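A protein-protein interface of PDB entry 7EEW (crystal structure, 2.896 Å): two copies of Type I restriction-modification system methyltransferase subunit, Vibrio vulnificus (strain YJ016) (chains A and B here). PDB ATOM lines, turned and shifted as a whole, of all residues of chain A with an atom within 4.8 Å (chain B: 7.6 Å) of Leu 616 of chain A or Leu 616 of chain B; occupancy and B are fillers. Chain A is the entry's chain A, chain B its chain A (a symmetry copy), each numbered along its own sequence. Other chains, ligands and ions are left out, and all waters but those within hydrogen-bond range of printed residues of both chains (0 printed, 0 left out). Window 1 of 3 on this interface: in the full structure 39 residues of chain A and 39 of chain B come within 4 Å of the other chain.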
ATOM      1  N   LEU A 445     -10.553  28.070  23.396  1.00  0.00           N
ATOM      2  CA  LEU A 445     -11.679  27.344  22.818  1.00  0.00           C
ATOM      3  C   LEU A 445     -11.228  25.999  22.260  1.00  0.00           C
ATOM      4  O   LEU A 445     -11.779  24.950  22.613  1.00  0.00           O
ATOM      5  CB  LEU A 445     -12.342  28.193  21.731  1.00  0.00           C
ATOM      6  CG  LEU A 445     -13.837  27.993  21.460  1.00  0.00           C
ATOM      7  CD1 LEU A 445     -14.090  26.786  20.572  1.00  0.00           C
ATOM      8  CD2 LEU A 445     -14.599  27.867  22.770  1.00  0.00           C
ATOM      9  N   ILE A 612     -17.214  23.385  28.463  1.00  0.00           N
ATOM     10  CA  ILE A 612     -16.991  23.828  27.089  1.00  0.00           C
ATOM     11  C   ILE A 612     -18.230  24.531  26.543  1.00  0.00           C
ATOM     12  O   ILE A 612     -18.127  25.570  25.879  1.00  0.00           O
ATOM     13  CB  ILE A 612     -16.562  22.641  26.204  1.00  0.00           C
ATOM     14  CG1 ILE A 612     -15.036  22.501  26.186  1.00  0.00           C
ATOM     15  CG2 ILE A 612     -17.085  22.798  24.783  1.00  0.00           C
ATOM     16  CD1 ILE A 612     -14.412  22.191  27.530  1.00  0.00           C
ATOM     17  N   GLN A 613     -19.418  23.988  26.820  1.00  0.00           N
ATOM     18  CA  GLN A 613     -20.644  24.658  26.396  1.00  0.00           C
ATOM     19  C   GLN A 613     -20.827  25.985  27.123  1.00  0.00           C
ATOM     20  O   GLN A 613     -21.337  26.951  26.543  1.00  0.00           O
ATOM     21  CB  GLN A 613     -21.852  23.752  26.628  1.00  0.00           C
ATOM     22  CG  GLN A 613     -21.936  22.568  25.681  1.00  0.00           C
ATOM     23  CD  GLN A 613     -23.228  21.792  25.839  1.00  0.00           C
ATOM     24  OE1 GLN A 613     -23.920  21.913  26.849  1.00  0.00           O
ATOM     25  NE2 GLN A 613     -23.562  20.991  24.834  1.00  0.00           N
ATOM     26  N   SER A 614     -20.420  26.049  28.393  1.00  0.00           N
ATOM     27  CA  SER A 614     -20.504  27.304  29.133  1.00  0.00           C
ATOM     28  C   SER A 614     -19.579  28.356  28.534  1.00  0.00           C
ATOM     29  O   SER A 614     -19.966  29.521  28.386  1.00  0.00           O
ATOM     30  CB  SER A 614     -20.169  27.073  30.605  1.00  0.00           C
ATOM     31  OG  SER A 614     -20.158  28.294  31.324  1.00  0.00           O
ATOM     32  N   LEU A 615     -18.353  27.964  28.183  1.00  0.00           N
ATOM     33  CA  LEU A 615     -17.442  28.903  27.540  1.00  0.00           C
ATOM     34  C   LEU A 615     -17.891  29.234  26.124  1.00  0.00           C
ATOM     35  O   LEU A 615     -17.628  30.337  25.635  1.00  0.00           O
ATOM     36  CB  LEU A 615     -16.020  28.342  27.533  1.00  0.00           C
ATOM     37  CG  LEU A 615     -15.405  28.063  28.908  1.00  0.00           C
ATOM     38  CD1 LEU A 615     -13.930  27.720  28.776  1.00  0.00           C
ATOM     39  CD2 LEU A 615     -15.609  29.243  29.845  1.00  0.00           C
ATOM     40  N   LEU A 616     -18.570  28.298  25.454  1.00  0.00           N
ATOM     41  CA  LEU A 616     -19.142  28.600  24.147  1.00  0.00           C
ATOM     42  C   LEU A 616     -20.224  29.667  24.255  1.00  0.00           C
ATOM     43  O   LEU A 616     -20.303  30.568  23.411  1.00  0.00           O
ATOM     44  CB  LEU A 616     -19.709  27.332  23.509  1.00  0.00           C
ATOM     45  CG  LEU A 616     -18.728  26.423  22.769  1.00  0.00           C
ATOM     46  CD1 LEU A 616     -19.461  25.224  22.192  1.00  0.00           C
ATOM     47  CD2 LEU A 616     -18.013  27.193  21.673  1.00  0.00           C
ATOM     48  N   ALA A 617     -21.069  29.582  25.286  1.00  0.00           N
ATOM     49  CA  ALA A 617     -22.110  30.585  25.473  1.00  0.00           C
ATOM     50  C   ALA A 617     -21.508  31.953  25.760  1.00  0.00           C
ATOM     51  O   ALA A 617     -21.971  32.970  25.228  1.00  0.00           O
ATOM     52  CB  ALA A 617     -23.052  30.163  26.601  1.00  0.00           C
ATOM     53  N   ASP A 618     -20.470  32.000  26.597  1.00  0.00           N
ATOM     54  CA  ASP A 618     -19.773  33.259  26.837  1.00  0.00           C
ATOM     55  C   ASP A 618     -19.094  33.754  25.568  1.00  0.00           C
ATOM     56  O   ASP A 618     -19.155  34.945  25.244  1.00  0.00           O
ATOM     57  CB  ASP A 618     -18.752  33.089  27.964  1.00  0.00           C
ATOM     58  CG  ASP A 618     -19.394  32.689  29.279  1.00  0.00           C
ATOM     59  OD1 ASP A 618     -20.607  32.391  29.286  1.00  0.00           O
ATOM     60  OD2 ASP A 618     -18.685  32.675  30.308  1.00  0.00           O
ATOM     61  N   PHE A 619     -18.451  32.847  24.828  1.00  0.00           N
ATOM     62  CA  PHE A 619     -17.784  33.234  23.590  1.00  0.00           C
ATOM     63  C   PHE A 619     -18.783  33.625  22.508  1.00  0.00           C
ATOM     64  O   PHE A 619     -18.472  34.464  21.657  1.00  0.00           O
ATOM     65  CB  PHE A 619     -16.890  32.094  23.103  1.00  0.00           C
ATOM     66  CG  PHE A 619     -16.072  32.435  21.890  1.00  0.00           C
ATOM     67  CD1 PHE A 619     -14.827  33.028  22.025  1.00  0.00           C
ATOM     68  CD2 PHE A 619     -16.542  32.155  20.618  1.00  0.00           C
ATOM     69  CE1 PHE A 619     -14.070  33.341  20.911  1.00  0.00           C
ATOM     70  CE2 PHE A 619     -15.791  32.466  19.502  1.00  0.00           C
ATOM     71  CZ  PHE A 619     -14.552  33.059  19.649  1.00  0.00           C
ATOM     72  N   SER A 620     -19.978  33.032  22.521  1.00  0.00           N
ATOM     73  CA  SER A 620     -20.968  33.343  21.494  1.00  0.00           C
ATOM     74  C   SER A 620     -21.458  34.781  21.620  1.00  0.00           C
ATOM     75  O   SER A 620     -21.504  35.521  20.630  1.00  0.00           O
ATOM     76  CB  SER A 620     -22.140  32.364  21.580  1.00  0.00           C
ATOM     77  OG  SER A 620     -23.113  32.639  20.588  1.00  0.00           O
ATOM     78  N   GLN B 442     -15.685  21.369  13.780  1.00  0.00           N
ATOM     79  CA  GLN B 442     -14.623  22.175  14.368  1.00  0.00           C
ATOM     80  C   GLN B 442     -13.693  22.726  13.298  1.00  0.00           C
ATOM     81  O   GLN B 442     -13.165  23.835  13.445  1.00  0.00           O
ATOM     82  CB  GLN B 442     -13.841  21.350  15.389  1.00  0.00           C
ATOM     83  CG  GLN B 442     -12.677  22.092  16.025  1.00  0.00           C
ATOM     84  CD  GLN B 442     -13.107  23.368  16.724  1.00  0.00           C
ATOM     85  OE1 GLN B 442     -14.262  23.517  17.123  1.00  0.00           O
ATOM     86  NE2 GLN B 442     -12.173  24.297  16.882  1.00  0.00           N
ATOM     87  N   LEU B 445     -15.549  25.452  12.208  1.00  0.00           N
ATOM     88  CA  LEU B 445     -15.687  26.416  13.295  1.00  0.00           C
ATOM     89  C   LEU B 445     -14.588  27.469  13.229  1.00  0.00           C
ATOM     90  O   LEU B 445     -14.865  28.674  13.209  1.00  0.00           O
ATOM     91  CB  LEU B 445     -15.667  25.688  14.641  1.00  0.00           C
ATOM     92  CG  LEU B 445     -16.424  26.311  15.818  1.00  0.00           C
ATOM     93  CD1 LEU B 445     -15.618  27.414  16.483  1.00  0.00           C
ATOM     94  CD2 LEU B 445     -17.776  26.834  15.359  1.00  0.00           C
ATOM     95  N   ILE B 449     -14.297  31.859  11.831  1.00  0.00           N
ATOM     96  CA  ILE B 449     -14.068  32.845  12.884  1.00  0.00           C
ATOM     97  C   ILE B 449     -12.705  33.505  12.725  1.00  0.00           C
ATOM     98  O   ILE B 449     -12.539  34.687  13.049  1.00  0.00           O
ATOM     99  CB  ILE B 449     -14.231  32.198  14.273  1.00  0.00           C
ATOM    100  CG1 ILE B 449     -13.213  31.077  14.466  1.00  0.00           C
ATOM    101  CG2 ILE B 449     -15.646  31.672  14.455  1.00  0.00           C
ATOM    102  CD1 ILE B 449     -13.475  30.221  15.675  1.00  0.00           C
ATOM    103  N   LYS B 609     -21.494  37.348  11.876  1.00  0.00           N
ATOM    104  CA  LYS B 609     -21.874  37.243  13.282  1.00  0.00           C
ATOM    105  C   LYS B 609     -23.087  36.336  13.458  1.00  0.00           C
ATOM    106  O   LYS B 609     -23.108  35.469  14.340  1.00  0.00           O
ATOM    107  CB  LYS B 609     -22.157  38.631  13.855  1.00  0.00           C
ATOM    108  CG  LYS B 609     -22.771  38.611  15.243  1.00  0.00           C
ATOM    109  CD  LYS B 609     -23.717  39.786  15.445  1.00  0.00           C
ATOM    110  CE  LYS B 609     -24.498  39.652  16.741  1.00  0.00           C
ATOM    111  NZ  LYS B 609     -25.577  40.672  16.851  1.00  0.00           N
ATOM    112  N   SER B 610     -24.109  36.519  12.618  1.00  0.00           N
ATOM    113  CA  SER B 610     -25.309  35.694  12.722  1.00  0.00           C
ATOM    114  C   SER B 610     -25.016  34.243  12.366  1.00  0.00           C
ATOM    115  O   SER B 610     -25.537  33.323  13.007  1.00  0.00           O
ATOM    116  CB  SER B 610     -26.414  36.254  11.823  1.00  0.00           C
ATOM    117  OG  SER B 610     -26.826  37.539  12.253  1.00  0.00           O
ATOM    118  N   LYS B 611     -24.180  34.020  11.352  1.00  0.00           N
ATOM    119  CA  LYS B 611     -23.891  32.660  10.911  1.00  0.00           C
ATOM    120  C   LYS B 611     -22.998  31.927  11.905  1.00  0.00           C
ATOM    121  O   LYS B 611     -23.253  30.761  12.234  1.00  0.00           O
ATOM    122  CB  LYS B 611     -23.249  32.696   9.524  1.00  0.00           C
ATOM    123  CG  LYS B 611     -22.249  31.588   9.256  1.00  0.00           C
ATOM    124  CD  LYS B 611     -21.395  31.927   8.048  1.00  0.00           C
ATOM    125  CE  LYS B 611     -20.208  30.989   7.923  1.00  0.00           C
ATOM    126  NZ  LYS B 611     -19.273  31.432   6.851  1.00  0.00           N
ATOM    127  N   ILE B 612     -21.951  32.591  12.400  1.00  0.00           N
ATOM    128  CA  ILE B 612     -21.017  31.931  13.307  1.00  0.00           C
ATOM    129  C   ILE B 612     -21.701  31.589  14.627  1.00  0.00           C
ATOM    130  O   ILE B 612     -21.511  30.495  15.174  1.00  0.00           O
ATOM    131  CB  ILE B 612     -19.762  32.801  13.514  1.00  0.00           C
ATOM    132  CG1 ILE B 612     -18.682  32.452  12.483  1.00  0.00           C
ATOM    133  CG2 ILE B 612     -19.206  32.639  14.923  1.00  0.00           C
ATOM    134  CD1 ILE B 612     -19.070  32.718  11.045  1.00  0.00           C
ATOM    135  N   GLN B 613     -22.513  32.508  15.156  1.00  0.00           N
ATOM    136  CA  GLN B 613     -23.260  32.208  16.374  1.00  0.00           C
ATOM    137  C   GLN B 613     -24.287  31.109  16.135  1.00  0.00           C
ATOM    138  O   GLN B 613     -24.543  30.287  17.023  1.00  0.00           O
ATOM    139  CB  GLN B 613     -23.942  33.470  16.903  1.00  0.00           C
ATOM    140  CG  GLN B 613     -22.990  34.490  17.500  1.00  0.00           C
ATOM    141  CD  GLN B 613     -23.718  35.646  18.156  1.00  0.00           C
ATOM    142  OE1 GLN B 613     -24.899  35.877  17.900  1.00  0.00           O
ATOM    143  NE2 GLN B 613     -23.015  36.377  19.012  1.00  0.00           N
ATOM    144  N   SER B 614     -24.889  31.081  14.943  1.00  0.00           N
ATOM    145  CA  SER B 614     -25.836  30.020  14.618  1.00  0.00           C
ATOM    146  C   SER B 614     -25.144  28.665  14.566  1.00  0.00           C
ATOM    147  O   SER B 614     -25.669  27.670  15.081  1.00  0.00           O
ATOM    148  CB  SER B 614     -26.530  30.319  13.290  1.00  0.00           C
ATOM    149  OG  SER B 614     -27.389  29.257  12.913  1.00  0.00           O
ATOM    150  N   LEU B 615     -23.963  28.604  13.948  1.00  0.00           N
ATOM    151  CA  LEU B 615     -23.214  27.353  13.923  1.00  0.00           C
ATOM    152  C   LEU B 615     -22.668  27.005  15.300  1.00  0.00           C
ATOM    153  O   LEU B 615     -22.509  25.822  15.619  1.00  0.00           O
ATOM    154  CB  LEU B 615     -22.081  27.434  12.901  1.00  0.00           C
ATOM    155  CG  LEU B 615     -22.505  27.678  11.450  1.00  0.00           C
ATOM    156  CD1 LEU B 615     -21.320  27.521  10.511  1.00  0.00           C
ATOM    157  CD2 LEU B 615     -23.643  26.750  11.052  1.00  0.00           C
ATOM    158  N   LEU B 616     -22.378  28.013  16.127  1.00  0.00           N
ATOM    159  CA  LEU B 616     -21.978  27.743  17.503  1.00  0.00           C
ATOM    160  C   LEU B 616     -23.110  27.092  18.286  1.00  0.00           C
ATOM    161  O   LEU B 616     -22.879  26.163  19.068  1.00  0.00           O
ATOM    162  CB  LEU B 616     -21.530  29.034  18.189  1.00  0.00           C
ATOM    163  CG  LEU B 616     -20.091  29.488  17.954  1.00  0.00           C
ATOM    164  CD1 LEU B 616     -19.817  30.774  18.716  1.00  0.00           C
ATOM    165  CD2 LEU B 616     -19.116  28.400  18.370  1.00  0.00           C
ATOM    166  N   ALA B 617     -24.343  27.568  18.091  1.00  0.00           N
ATOM    167  CA  ALA B 617     -25.482  26.975  18.782  1.00  0.00           C
ATOM    168  C   ALA B 617     -25.701  25.534  18.341  1.00  0.00           C
ATOM    169  O   ALA B 617     -25.972  24.656  19.168  1.00  0.00           O
ATOM    170  CB  ALA B 617     -26.739  27.809  18.539  1.00  0.00           C
ATOM    171  N   ASP B 618     -25.582  25.270  17.037  1.00  0.00           N
ATOM    172  CA  ASP B 618     -25.672  23.897  16.553  1.00  0.00           C
ATOM    173  C   ASP B 618     -24.518  23.058  17.084  1.00  0.00           C
ATOM    174  O   ASP B 618     -24.716  21.915  17.513  1.00  0.00           O
ATOM    175  CB  ASP B 618     -25.692  23.878  15.023  1.00  0.00           C
ATOM    176  CG  ASP B 618     -26.881  24.623  14.445  1.00  0.00           C
ATOM    177  OD1 ASP B 618     -27.605  25.285  15.218  1.00  0.00           O
ATOM    178  OD2 ASP B 618     -27.093  24.543  13.217  1.00  0.00           O
ATOM    179  N   PHE B 619     -23.305  23.616  17.078  1.00  0.00           N
ATOM    180  CA  PHE B 619     -22.147  22.886  17.580  1.00  0.00           C
ATOM    181  C   PHE B 619     -22.212  22.695  19.091  1.00  0.00           C
ATOM    182  O   PHE B 619     -21.694  21.700  19.609  1.00  0.00           O
ATOM    183  CB  PHE B 619     -20.862  23.617  17.191  1.00  0.00           C
ATOM    184  CG  PHE B 619     -19.606  22.886  17.568  1.00  0.00           C
ATOM    185  CD1 PHE B 619     -19.048  21.955  16.708  1.00  0.00           C
ATOM    186  CD2 PHE B 619     -18.978  23.136  18.777  1.00  0.00           C
ATOM    187  CE1 PHE B 619     -17.890  21.282  17.050  1.00  0.00           C
ATOM    188  CE2 PHE B 619     -17.821  22.467  19.125  1.00  0.00           C
ATOM    189  CZ  PHE B 619     -17.276  21.539  18.260  1.00  0.00           C
ATOM    190  N   SER B 620     -22.836  23.630  19.810  1.00  0.00           N
ATOM    191  CA  SER B 620     -22.906  23.518  21.265  1.00  0.00           C
ATOM    192  C   SER B 620     -23.771  22.334  21.684  1.00  0.00           C
ATOM    193  O   SER B 620     -23.368  21.528  22.530  1.00  0.00           O
ATOM    194  CB  SER B 620     -23.442  24.818  21.866  1.00  0.00           C
ATOM    195  OG  SER B 620     -23.514  24.739  23.278  1.00  0.00           O
ATOM    196  N   ARG B 621     -24.962  22.210  21.098  1.00  0.00           N
ATOM    197  CA  ARG B 621     -25.854  21.111  21.448  1.00  0.00           C
ATOM    198  C   ARG B 621     -25.393  19.786  20.852  1.00  0.00           C
ATOM    199  O   ARG B 621     -25.631  18.728  21.448  1.00  0.00           O
ATOM    200  CB  ARG B 621     -27.282  21.425  20.995  1.00  0.00           C
ATOM    201  CG  ARG B 621     -27.421  21.626  19.496  1.00  0.00           C
ATOM    202  CD  ARG B 621     -28.828  21.308  19.023  1.00  0.00           C
ATOM    203  NE  ARG B 621     -28.837  20.844  17.639  1.00  0.00           N
ATOM    204  CZ  ARG B 621     -29.082  21.620  16.589  1.00  0.00           C
ATOM    205  NH1 ARG B 621     -29.068  21.107  15.366  1.00  0.00           N
ATOM    206  NH2 ARG B 621     -29.347  22.908  16.761  1.00  0.00           N
ATOM    207  N   ASN B 622     -24.734  19.815  19.689  1.00  0.00           N
ATOM    208  CA  ASN B 622     -24.266  18.572  19.084  1.00  0.00           C
ATOM    209  C   ASN B 622     -23.144  17.941  19.898  1.00  0.00           C
ATOM    210  O   ASN B 622     -23.052  16.711  19.969  1.00  0.00           O
ATOM    211  CB  ASN B 622     -23.807  18.815  17.647  1.00  0.00           C
ATOM    212  CG  ASN B 622     -24.969  18.999  16.686  1.00  0.00           C
ATOM    213  OD1 ASN B 622     -26.100  18.602  16.975  1.00  0.00           O
ATOM    214  ND2 ASN B 622     -24.695  19.598  15.533  1.00  0.00           N
ATOM    215  N   LEU B 623     -22.287  18.756  20.513  1.00  0.00           N
ATOM    216  CA  LEU B 623     -21.279  18.205  21.410  1.00  0.00           C
ATOM    217  C   LEU B 623     -21.914  17.644  22.675  1.00  0.00           C
ATOM    218  O   LEU B 623     -21.388  16.690  23.261  1.00  0.00           O
ATOM    219  CB  LEU B 623     -20.240  19.272  21.759  1.00  0.00           C
ATOM    220  CG  LEU B 623     -19.062  18.830  22.630  1.00  0.00           C
ATOM    221  CD1 LEU B 623     -17.752  19.330  22.046  1.00  0.00           C
ATOM    222  CD2 LEU B 623     -19.226  19.316  24.064  1.00  0.00           C
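The side-chain amide nitrogen (NE2) of Gln 613 of chain A sits close to the backbone carbonyl oxygen (O) of Ser 620 of chain B (2.4 Å). The backbone carbonyl oxygen (O) of Ser 620 of chain A sits close to the side-chain amide nitrogen (NE2) of Gln 613 of chain B.
Among the printed residues, merely in contact across the chains: Leu 616 of chain A with Leu 616 of chain B (3.7 Å), Leu 616 of chain A with Ser 620 of chain B (3.95 Å) and Ser 620 of chain A with Leu 616 of chain B (3.95 Å).
Of the printed residues of chain B, Gln 613 of chain A touches Ser 620. Ser 610 of chain B touches none of the printed residues of chain A. Printed residues of chain A within 4 Å of Gln 613 of chain B: Ser 620. Printed residues of chain A within 4 Å of Leu 616 of chain B: Leu 616 and Ser 620. The nearest residue of chain B that does not touch Leu 616 of chain A is Phe 619 of chain B (4.03 Å). The nearest printed residue of chain B that does not touch Gln 613 of chain A is Arg 621 of chain B (4.1 Å).
Of the 18 printed residues of chain B, 3 touch a printed residue of chain A. Printed residues of chain B that touch a printed residue of chain A: Gln 613, Leu 616 and Ser 620. Of the 10 printed residues of chain A, 3 touch a printed residue of chain B. Hydrophobic or aromatic side chains of chain A within 4 Å of the printed part of chain B: Leu 616. Among the printed residues, no Asp or Glu carboxylate lies within 4 Å of a Lys or Arg side-chain nitrogen of the other chain.
Gln 613 of chain A touches Ser 620 of chain B, and with the chains exchanged Ser 620 of chain A touches Gln 613 of chain B. Leu 616 of chain A touches its own counterpart, Leu 616 of chain B. Leu 616 of chain A touches Ser 620 of chain B, and with the chains exchanged Ser 620 of chain A touches Leu 616 of chain B.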
